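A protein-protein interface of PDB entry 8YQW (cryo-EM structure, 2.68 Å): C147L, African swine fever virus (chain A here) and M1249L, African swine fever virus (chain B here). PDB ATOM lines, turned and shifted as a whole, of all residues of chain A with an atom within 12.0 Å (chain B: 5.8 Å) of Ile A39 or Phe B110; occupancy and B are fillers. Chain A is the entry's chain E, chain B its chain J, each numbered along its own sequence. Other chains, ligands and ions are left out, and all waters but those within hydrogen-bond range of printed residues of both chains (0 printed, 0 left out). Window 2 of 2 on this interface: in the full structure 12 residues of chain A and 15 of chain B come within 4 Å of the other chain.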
ATOM      1  N   ILE A  39      17.137  10.758 -21.773  1.00  0.00           N
ATOM      2  CA  ILE A  39      17.389  11.349 -20.463  1.00  0.00           C
ATOM      3  C   ILE A  39      16.243  12.267 -20.056  1.00  0.00           C
ATOM      4  O   ILE A  39      15.615  12.905 -20.901  1.00  0.00           O
ATOM      5  CB  ILE A  39      18.726  12.108 -20.445  1.00  0.00           C
ATOM      6  CG1 ILE A  39      18.748  13.174 -21.540  1.00  0.00           C
ATOM      7  CG2 ILE A  39      19.891  11.146 -20.604  1.00  0.00           C
ATOM      8  CD1 ILE A  39      19.899  14.140 -21.425  1.00  0.00           C
ATOM      9  N   VAL A  40      15.972  12.325 -18.755  1.00  0.00           N
ATOM     10  CA  VAL A  40      14.912  13.168 -18.213  1.00  0.00           C
ATOM     11  C   VAL A  40      15.566  14.460 -17.733  1.00  0.00           C
ATOM     12  O   VAL A  40      16.199  14.499 -16.677  1.00  0.00           O
ATOM     13  CB  VAL A  40      14.146  12.467 -17.092  1.00  0.00           C
ATOM     14  CG1 VAL A  40      13.048  13.374 -16.578  1.00  0.00           C
ATOM     15  CG2 VAL A  40      13.572  11.149 -17.587  1.00  0.00           C
ATOM     16  N   GLU A  41      15.406  15.520 -18.514  1.00  0.00           N
ATOM     17  CA  GLU A  41      16.094  16.778 -18.278  1.00  0.00           C
ATOM     18  C   GLU A  41      15.231  17.719 -17.437  1.00  0.00           C
ATOM     19  O   GLU A  41      14.230  17.319 -16.837  1.00  0.00           O
ATOM     20  CB  GLU A  41      16.500  17.395 -19.613  1.00  0.00           C
ATOM     21  CG  GLU A  41      15.339  17.637 -20.553  1.00  0.00           C
ATOM     22  CD  GLU A  41      15.800  18.047 -21.933  1.00  0.00           C
ATOM     23  OE1 GLU A  41      17.025  18.177 -22.133  1.00  0.00           O
ATOM     24  OE2 GLU A  41      14.941  18.219 -22.821  1.00  0.00           O
ATOM     25  N   SER A  42      15.630  18.988 -17.383  1.00  0.00           N
ATOM     26  CA  SER A  42      14.989  19.969 -16.528  1.00  0.00           C
ATOM     27  C   SER A  42      13.545  20.211 -16.965  1.00  0.00           C
ATOM     28  O   SER A  42      13.198  20.012 -18.131  1.00  0.00           O
ATOM     29  CB  SER A  42      15.777  21.276 -16.564  1.00  0.00           C
ATOM     30  OG  SER A  42      17.118  21.071 -16.153  1.00  0.00           O
ATOM     31  N   PRO A  43      12.679  20.622 -16.035  1.00  0.00           N
ATOM     32  CA  PRO A  43      11.283  20.887 -16.400  1.00  0.00           C
ATOM     33  C   PRO A  43      11.171  21.996 -17.435  1.00  0.00           C
ATOM     34  O   PRO A  43      11.910  22.982 -17.406  1.00  0.00           O
ATOM     35  CB  PRO A  43      10.637  21.296 -15.069  1.00  0.00           C
ATOM     36  CG  PRO A  43      11.775  21.737 -14.212  1.00  0.00           C
ATOM     37  CD  PRO A  43      12.928  20.868 -14.605  1.00  0.00           C
ATOM     38  N   SER A  44      10.227  21.824 -18.351  1.00  0.00           N
ATOM     39  CA  SER A  44      10.008  22.746 -19.453  1.00  0.00           C
ATOM     40  C   SER A  44       8.703  23.509 -19.245  1.00  0.00           C
ATOM     41  O   SER A  44       7.885  23.173 -18.386  1.00  0.00           O
ATOM     42  CB  SER A  44      10.002  21.993 -20.786  1.00  0.00           C
ATOM     43  OG  SER A  44       8.982  21.008 -20.811  1.00  0.00           O
ATOM     44  N   CYS A  46       6.280  23.554 -21.305  1.00  0.00           N
ATOM     45  CA  CYS A  46       5.147  22.784 -21.809  1.00  0.00           C
ATOM     46  C   CYS A  46       4.370  22.128 -20.672  1.00  0.00           C
ATOM     47  O   CYS A  46       3.146  21.981 -20.753  1.00  0.00           O
ATOM     48  CB  CYS A  46       5.624  21.744 -22.822  1.00  0.00           C
ATOM     49  SG  CYS A  46       6.827  20.556 -22.196  1.00  0.00           S
ATOM     50  N   GLU A  47       5.060  21.724 -19.610  1.00  0.00           N
ATOM     51  CA  GLU A  47       4.381  21.377 -18.372  1.00  0.00           C
ATOM     52  C   GLU A  47       4.539  22.512 -17.363  1.00  0.00           C
ATOM     53  O   GLU A  47       5.161  23.541 -17.636  1.00  0.00           O
ATOM     54  CB  GLU A  47       4.905  20.060 -17.793  1.00  0.00           C
ATOM     55  CG  GLU A  47       6.335  20.093 -17.280  1.00  0.00           C
ATOM     56  CD  GLU A  47       7.314  19.452 -18.242  1.00  0.00           C
ATOM     57  OE1 GLU A  47       6.959  19.286 -19.423  1.00  0.00           O
ATOM     58  OE2 GLU A  47       8.434  19.106 -17.813  1.00  0.00           O
ATOM     59  N   PRO B  90      23.179  22.239 -22.434  1.00  0.00           N
ATOM     60  CA  PRO B  90      24.168  21.698 -21.500  1.00  0.00           C
ATOM     61  C   PRO B  90      25.554  21.702 -22.125  1.00  0.00           C
ATOM     62  O   PRO B  90      25.712  21.813 -23.342  1.00  0.00           O
ATOM     63  CB  PRO B  90      23.659  20.272 -21.263  1.00  0.00           C
ATOM     64  CG  PRO B  90      23.087  19.940 -22.611  1.00  0.00           C
ATOM     65  CD  PRO B  90      22.247  21.175 -22.845  1.00  0.00           C
ATOM     66  N   ILE B  91      26.565  21.577 -21.273  1.00  0.00           N
ATOM     67  CA  ILE B  91      27.954  21.711 -21.693  1.00  0.00           C
ATOM     68  C   ILE B  91      28.687  20.401 -21.432  1.00  0.00           C
ATOM     69  O   ILE B  91      28.326  19.630 -20.536  1.00  0.00           O
ATOM     70  CB  ILE B  91      28.640  22.888 -20.966  1.00  0.00           C
ATOM     71  CG1 ILE B  91      27.798  24.158 -21.085  1.00  0.00           C
ATOM     72  CG2 ILE B  91      30.010  23.154 -21.546  1.00  0.00           C
ATOM     73  CD1 ILE B  91      26.937  24.447 -19.877  1.00  0.00           C
ATOM     74  N   VAL B  92      29.720  20.146 -22.232  1.00  0.00           N
ATOM     75  CA  VAL B  92      30.579  18.977 -22.083  1.00  0.00           C
ATOM     76  C   VAL B  92      31.912  19.432 -21.500  1.00  0.00           C
ATOM     77  O   VAL B  92      32.444  20.483 -21.884  1.00  0.00           O
ATOM     78  CB  VAL B  92      30.768  18.233 -23.419  1.00  0.00           C
ATOM     79  CG1 VAL B  92      29.436  17.687 -23.904  1.00  0.00           C
ATOM     80  CG2 VAL B  92      31.369  19.144 -24.467  1.00  0.00           C
ATOM     81  N   SER B  93      32.433  18.658 -20.553  1.00  0.00           N
ATOM     82  CA  SER B  93      33.621  19.028 -19.799  1.00  0.00           C
ATOM     83  C   SER B  93      34.717  17.986 -19.969  1.00  0.00           C
ATOM     84  O   SER B  93      34.463  16.780 -19.886  1.00  0.00           O
ATOM     85  CB  SER B  93      33.289  19.197 -18.314  1.00  0.00           C
ATOM     86  OG  SER B  93      32.860  17.972 -17.745  1.00  0.00           O
ATOM     87  N   GLU B 108      23.423  21.403 -15.090  1.00  0.00           N
ATOM     88  CA  GLU B 108      23.582  20.006 -15.466  1.00  0.00           C
ATOM     89  C   GLU B 108      24.436  19.937 -16.724  1.00  0.00           C
ATOM     90  O   GLU B 108      24.009  20.380 -17.795  1.00  0.00           O
ATOM     91  CB  GLU B 108      22.225  19.343 -15.692  1.00  0.00           C
ATOM     92  CG  GLU B 108      21.299  19.410 -14.494  1.00  0.00           C
ATOM     93  CD  GLU B 108      20.069  18.540 -14.660  1.00  0.00           C
ATOM     94  OE1 GLU B 108      20.048  17.706 -15.588  1.00  0.00           O
ATOM     95  OE2 GLU B 108      19.124  18.689 -13.860  1.00  0.00           O
ATOM     96  N   ILE B 109      25.642  19.389 -16.592  1.00  0.00           N
ATOM     97  CA  ILE B 109      26.595  19.312 -17.684  1.00  0.00           C
ATOM     98  C   ILE B 109      26.889  17.845 -17.978  1.00  0.00           C
ATOM     99  O   ILE B 109      26.502  16.938 -17.234  1.00  0.00           O
ATOM    100  CB  ILE B 109      27.898  20.076 -17.379  1.00  0.00           C
ATOM    101  CG1 ILE B 109      28.635  19.426 -16.208  1.00  0.00           C
ATOM    102  CG2 ILE B 109      27.605  21.535 -17.077  1.00  0.00           C
ATOM    103  CD1 ILE B 109      30.138  19.570 -16.283  1.00  0.00           C
ATOM    104  N   PHE B 110      27.573  17.630 -19.095  1.00  0.00           N
ATOM    105  CA  PHE B 110      27.991  16.313 -19.534  1.00  0.00           C
ATOM    106  C   PHE B 110      29.509  16.231 -19.501  1.00  0.00           C
ATOM    107  O   PHE B 110      30.210  17.245 -19.442  1.00  0.00           O
ATOM    108  CB  PHE B 110      27.481  16.011 -20.949  1.00  0.00           C
ATOM    109  CG  PHE B 110      26.070  15.503 -20.993  1.00  0.00           C
ATOM    110  CD1 PHE B 110      25.789  14.171 -20.744  1.00  0.00           C
ATOM    111  CD2 PHE B 110      25.024  16.358 -21.295  1.00  0.00           C
ATOM    112  CE1 PHE B 110      24.489  13.704 -20.785  1.00  0.00           C
ATOM    113  CE2 PHE B 110      23.725  15.898 -21.341  1.00  0.00           C
ATOM    114  CZ  PHE B 110      23.456  14.569 -21.086  1.00  0.00           C
ATOM    115  N   LEU B 111      30.013  15.004 -19.528  1.00  0.00           N
ATOM    116  CA  LEU B 111      31.439  14.748 -19.622  1.00  0.00           C
ATOM    117  C   LEU B 111      31.735  14.049 -20.940  1.00  0.00           C
ATOM    118  O   LEU B 111      30.852  13.449 -21.558  1.00  0.00           O
ATOM    119  CB  LEU B 111      31.937  13.887 -18.451  1.00  0.00           C
ATOM    120  CG  LEU B 111      32.086  14.563 -17.087  1.00  0.00           C
ATOM    121  CD1 LEU B 111      30.773  14.538 -16.327  1.00  0.00           C
ATOM    122  CD2 LEU B 111      33.186  13.903 -16.276  1.00  0.00           C
ATOM    123  N   ILE B 112      32.992  14.147 -21.379  1.00  0.00           N
ATOM    124  CA  ILE B 112      33.433  13.307 -22.482  1.00  0.00           C
ATOM    125  C   ILE B 112      33.382  11.856 -22.029  1.00  0.00           C
ATOM    126  O   ILE B 112      33.778  11.526 -20.905  1.00  0.00           O
ATOM    127  CB  ILE B 112      34.839  13.707 -22.960  1.00  0.00           C
ATOM    128  CG1 ILE B 112      35.837  13.678 -21.802  1.00  0.00           C
ATOM    129  CG2 ILE B 112      34.804  15.077 -23.617  1.00  0.00           C
ATOM    130  CD1 ILE B 112      37.279  13.677 -22.245  1.00  0.00           C
ATOM    131  N   GLY B 114      30.305  10.749 -22.266  1.00  0.00           N
ATOM    132  CA  GLY B 114      28.870  10.797 -22.058  1.00  0.00           C
ATOM    133  C   GLY B 114      28.381  10.392 -20.683  1.00  0.00           C
ATOM    134  O   GLY B 114      27.735   9.351 -20.533  1.00  0.00           O
ATOM    135  N   THR B 115      28.679  11.200 -19.670  1.00  0.00           N
ATOM    136  CA  THR B 115      28.144  11.010 -18.329  1.00  0.00           C
ATOM    137  C   THR B 115      27.543  12.327 -17.858  1.00  0.00           C
ATOM    138  O   THR B 115      28.165  13.383 -18.009  1.00  0.00           O
ATOM    139  CB  THR B 115      29.225  10.531 -17.357  1.00  0.00           C
ATOM    140  OG1 THR B 115      29.978   9.476 -17.965  1.00  0.00           O
ATOM    141  CG2 THR B 115      28.588  10.000 -16.086  1.00  0.00           C
ATOM    142  N   HIS B 116      26.341  12.260 -17.291  1.00  0.00           N
ATOM    143  CA  HIS B 116      25.558  13.439 -16.940  1.00  0.00           C
ATOM    144  C   HIS B 116      25.693  13.721 -15.448  1.00  0.00           C
ATOM    145  O   HIS B 116      25.299  12.893 -14.621  1.00  0.00           O
ATOM    146  CB  HIS B 116      24.091  13.224 -17.311  1.00  0.00           C
ATOM    147  CG  HIS B 116      23.281  14.481 -17.352  1.00  0.00           C
ATOM    148  ND1 HIS B 116      21.904  14.476 -17.331  1.00  0.00           N
ATOM    149  CD2 HIS B 116      23.652  15.781 -17.418  1.00  0.00           C
ATOM    150  CE1 HIS B 116      21.460  15.719 -17.380  1.00  0.00           C
ATOM    151  NE2 HIS B 116      22.502  16.530 -17.433  1.00  0.00           N
ATOM    152  N   LEU B 117      26.240  14.889 -15.107  1.00  0.00           N
ATOM    153  CA  LEU B 117      26.389  15.280 -13.713  1.00  0.00           C
ATOM    154  C   LEU B 117      26.038  16.751 -13.562  1.00  0.00           C
ATOM    155  O   LEU B 117      26.206  17.540 -14.492  1.00  0.00           O
ATOM    156  CB  LEU B 117      27.814  15.041 -13.188  1.00  0.00           C
ATOM    157  CG  LEU B 117      28.168  13.673 -12.600  1.00  0.00           C
ATOM    158  CD1 LEU B 117      28.416  12.650 -13.688  1.00  0.00           C
ATOM    159  CD2 LEU B 117      29.378  13.787 -11.690  1.00  0.00           C
ATOM    160  N   ARG B 133      20.298  21.529 -27.007  1.00  0.00           N
ATOM    161  CA  ARG B 133      19.292  20.522 -27.303  1.00  0.00           C
ATOM    162  C   ARG B 133      18.089  21.189 -27.955  1.00  0.00           C
ATOM    163  O   ARG B 133      17.475  22.086 -27.368  1.00  0.00           O
ATOM    164  CB  ARG B 133      18.859  19.775 -26.043  1.00  0.00           C
ATOM    165  CG  ARG B 133      17.763  18.756 -26.308  1.00  0.00           C
ATOM    166  CD  ARG B 133      17.686  17.702 -25.221  1.00  0.00           C
ATOM    167  NE  ARG B 133      16.629  16.735 -25.489  1.00  0.00           N
ATOM    168  CZ  ARG B 133      16.580  15.513 -24.974  1.00  0.00           C
ATOM    169  NH1 ARG B 133      17.519  15.072 -24.152  1.00  0.00           N
ATOM    170  NH2 ARG B 133      15.563  14.716 -25.288  1.00  0.00           N
ATOM    171  N   TRP B 181      30.185  15.003 -31.118  1.00  0.00           N
ATOM    172  CA  TRP B 181      29.696  14.420 -29.878  1.00  0.00           C
ATOM    173  C   TRP B 181      28.232  14.071 -30.084  1.00  0.00           C
ATOM    174  O   TRP B 181      27.482  14.868 -30.653  1.00  0.00           O
ATOM    175  CB  TRP B 181      29.860  15.393 -28.706  1.00  0.00           C
ATOM    176  CG  TRP B 181      29.693  14.745 -27.376  1.00  0.00           C
ATOM    177  CD1 TRP B 181      30.497  13.789 -26.831  1.00  0.00           C
ATOM    178  CD2 TRP B 181      28.641  14.971 -26.434  1.00  0.00           C
ATOM    179  NE1 TRP B 181      30.023  13.421 -25.596  1.00  0.00           N
ATOM    180  CE2 TRP B 181      28.883  14.131 -25.330  1.00  0.00           C
ATOM    181  CE3 TRP B 181      27.524  15.808 -26.411  1.00  0.00           C
ATOM    182  CZ2 TRP B 181      28.049  14.102 -24.219  1.00  0.00           C
ATOM    183  CZ3 TRP B 181      26.699  15.778 -25.305  1.00  0.00           C
ATOM    184  CH2 TRP B 181      26.964  14.931 -24.227  1.00  0.00           C
ATOM    185  N   LYS B 183      24.583  11.970 -28.394  1.00  0.00           N
ATOM    186  CA  LYS B 183      23.841  11.305 -27.329  1.00  0.00           C
ATOM    187  C   LYS B 183      22.369  11.266 -27.727  1.00  0.00           C
ATOM    188  O   LYS B 183      22.019  11.476 -28.893  1.00  0.00           O
ATOM    189  CB  LYS B 183      24.064  11.984 -25.974  1.00  0.00           C
ATOM    190  CG  LYS B 183      24.170  10.982 -24.835  1.00  0.00           C
ATOM    191  CD  LYS B 183      24.623  11.621 -23.544  1.00  0.00           C
ATOM    192  CE  LYS B 183      24.655  10.594 -22.420  1.00  0.00           C
ATOM    193  NZ  LYS B 183      25.642   9.511 -22.680  1.00  0.00           N
ATOM    194  N   ASN B 184      21.505  10.980 -26.749  1.00  0.00           N
ATOM    195  CA  ASN B 184      20.076  10.833 -27.009  1.00  0.00           C
ATOM    196  C   ASN B 184      19.495  12.084 -27.659  1.00  0.00           C
ATOM    197  O   ASN B 184      18.997  12.040 -28.790  1.00  0.00           O
ATOM    198  CB  ASN B 184      19.343  10.520 -25.702  1.00  0.00           C
ATOM    199  CG  ASN B 184      17.839  10.402 -25.883  1.00  0.00           C
ATOM    200  OD1 ASN B 184      17.346  10.196 -26.993  1.00  0.00           O
ATOM    201  ND2 ASN B 184      17.101  10.544 -24.788  1.00  0.00           N
ATOM    202  N   GLY B 185      19.543  13.209 -26.950  1.00  0.00           N
ATOM    203  CA  GLY B 185      18.896  14.416 -27.439  1.00  0.00           C
ATOM    204  C   GLY B 185      19.557  14.935 -28.702  1.00  0.00           C
ATOM    205  O   GLY B 185      20.781  15.107 -28.757  1.00  0.00           O
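Among the printed residues, pairs that only touch across the chains: Ile A39 with Phe B110 (3.6 Å), Ile A39 with Arg B133 (3.5 Å) and Ser A42 with Glu B108 (3.9 Å).
Ile A39 touches just these residues of chain B: Phe B110, Arg B133 and Asn B184.
Phe B110 touches one residue of chain A.
No residue of chain A comes within 4 Å of Pro B90.
No residue of chain A comes within 4 Å of Ile B91.
No residue of chain A comes within 4 Å of Ser B93.
No residue of chain A comes within 4 Å of Ile B109.
No residue of chain A comes within 4 Å of Leu B111.
No residue of chain A comes within 4 Å of Gly B114.
No residue of chain A comes within 4 Å of His B116.
Of chain A, only Ile A39 comes within 4 Å of Asn B184.
Printed residues of chain A within 4 Å of Glu B108: Ser A42.
Of the printed residues of chain B, Glu A41 touches Arg B133.
Leu B117 touches none of the printed residues of chain A.
Ile B112 touches none of the printed residues of chain A.
The nearest residue of chain B that does not touch Ile A39 is His B116 (4.6 Å).
The nearest residue of chain A that does not touch Phe B110 is Glu A41 (7.1 Å).
The nearest printed residue of chain B that does not touch Glu A41 is Glu B108 (4.9 Å).
The backbone NH (N) of Phe B110 lies within hydrogen-bond range of the backbone carbonyl oxygen (O) of Ile B91, 2.6 Å away.
The backbone carbonyl oxygen of Phe B110 sits at hydrogen-bond distance from the backbone NH of Ser B93 (2.9 Å).
OE1 of Glu B108 sits close to NE2 of His B116, 3.3 Å away.
Hydrophobic or aromatic side chains of chain A that line the printed part of chain B: Ile A39.
Among the printed residues, 5 pairs touch across the chains.
Among the printed residues, Asp or Glu carboxylates within 4 Å of a Lys or Arg side-chain nitrogen of the other chain: Glu A41 with Arg B133.
N of Ile A39 sits close to ND2 of Asn B184 (3.0 Å).
The side-chain carboxylate (OE2) of Glu A41 lies within salt-bridge range of the guanidinium group (NE) of Arg B133 (3.5 Å).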
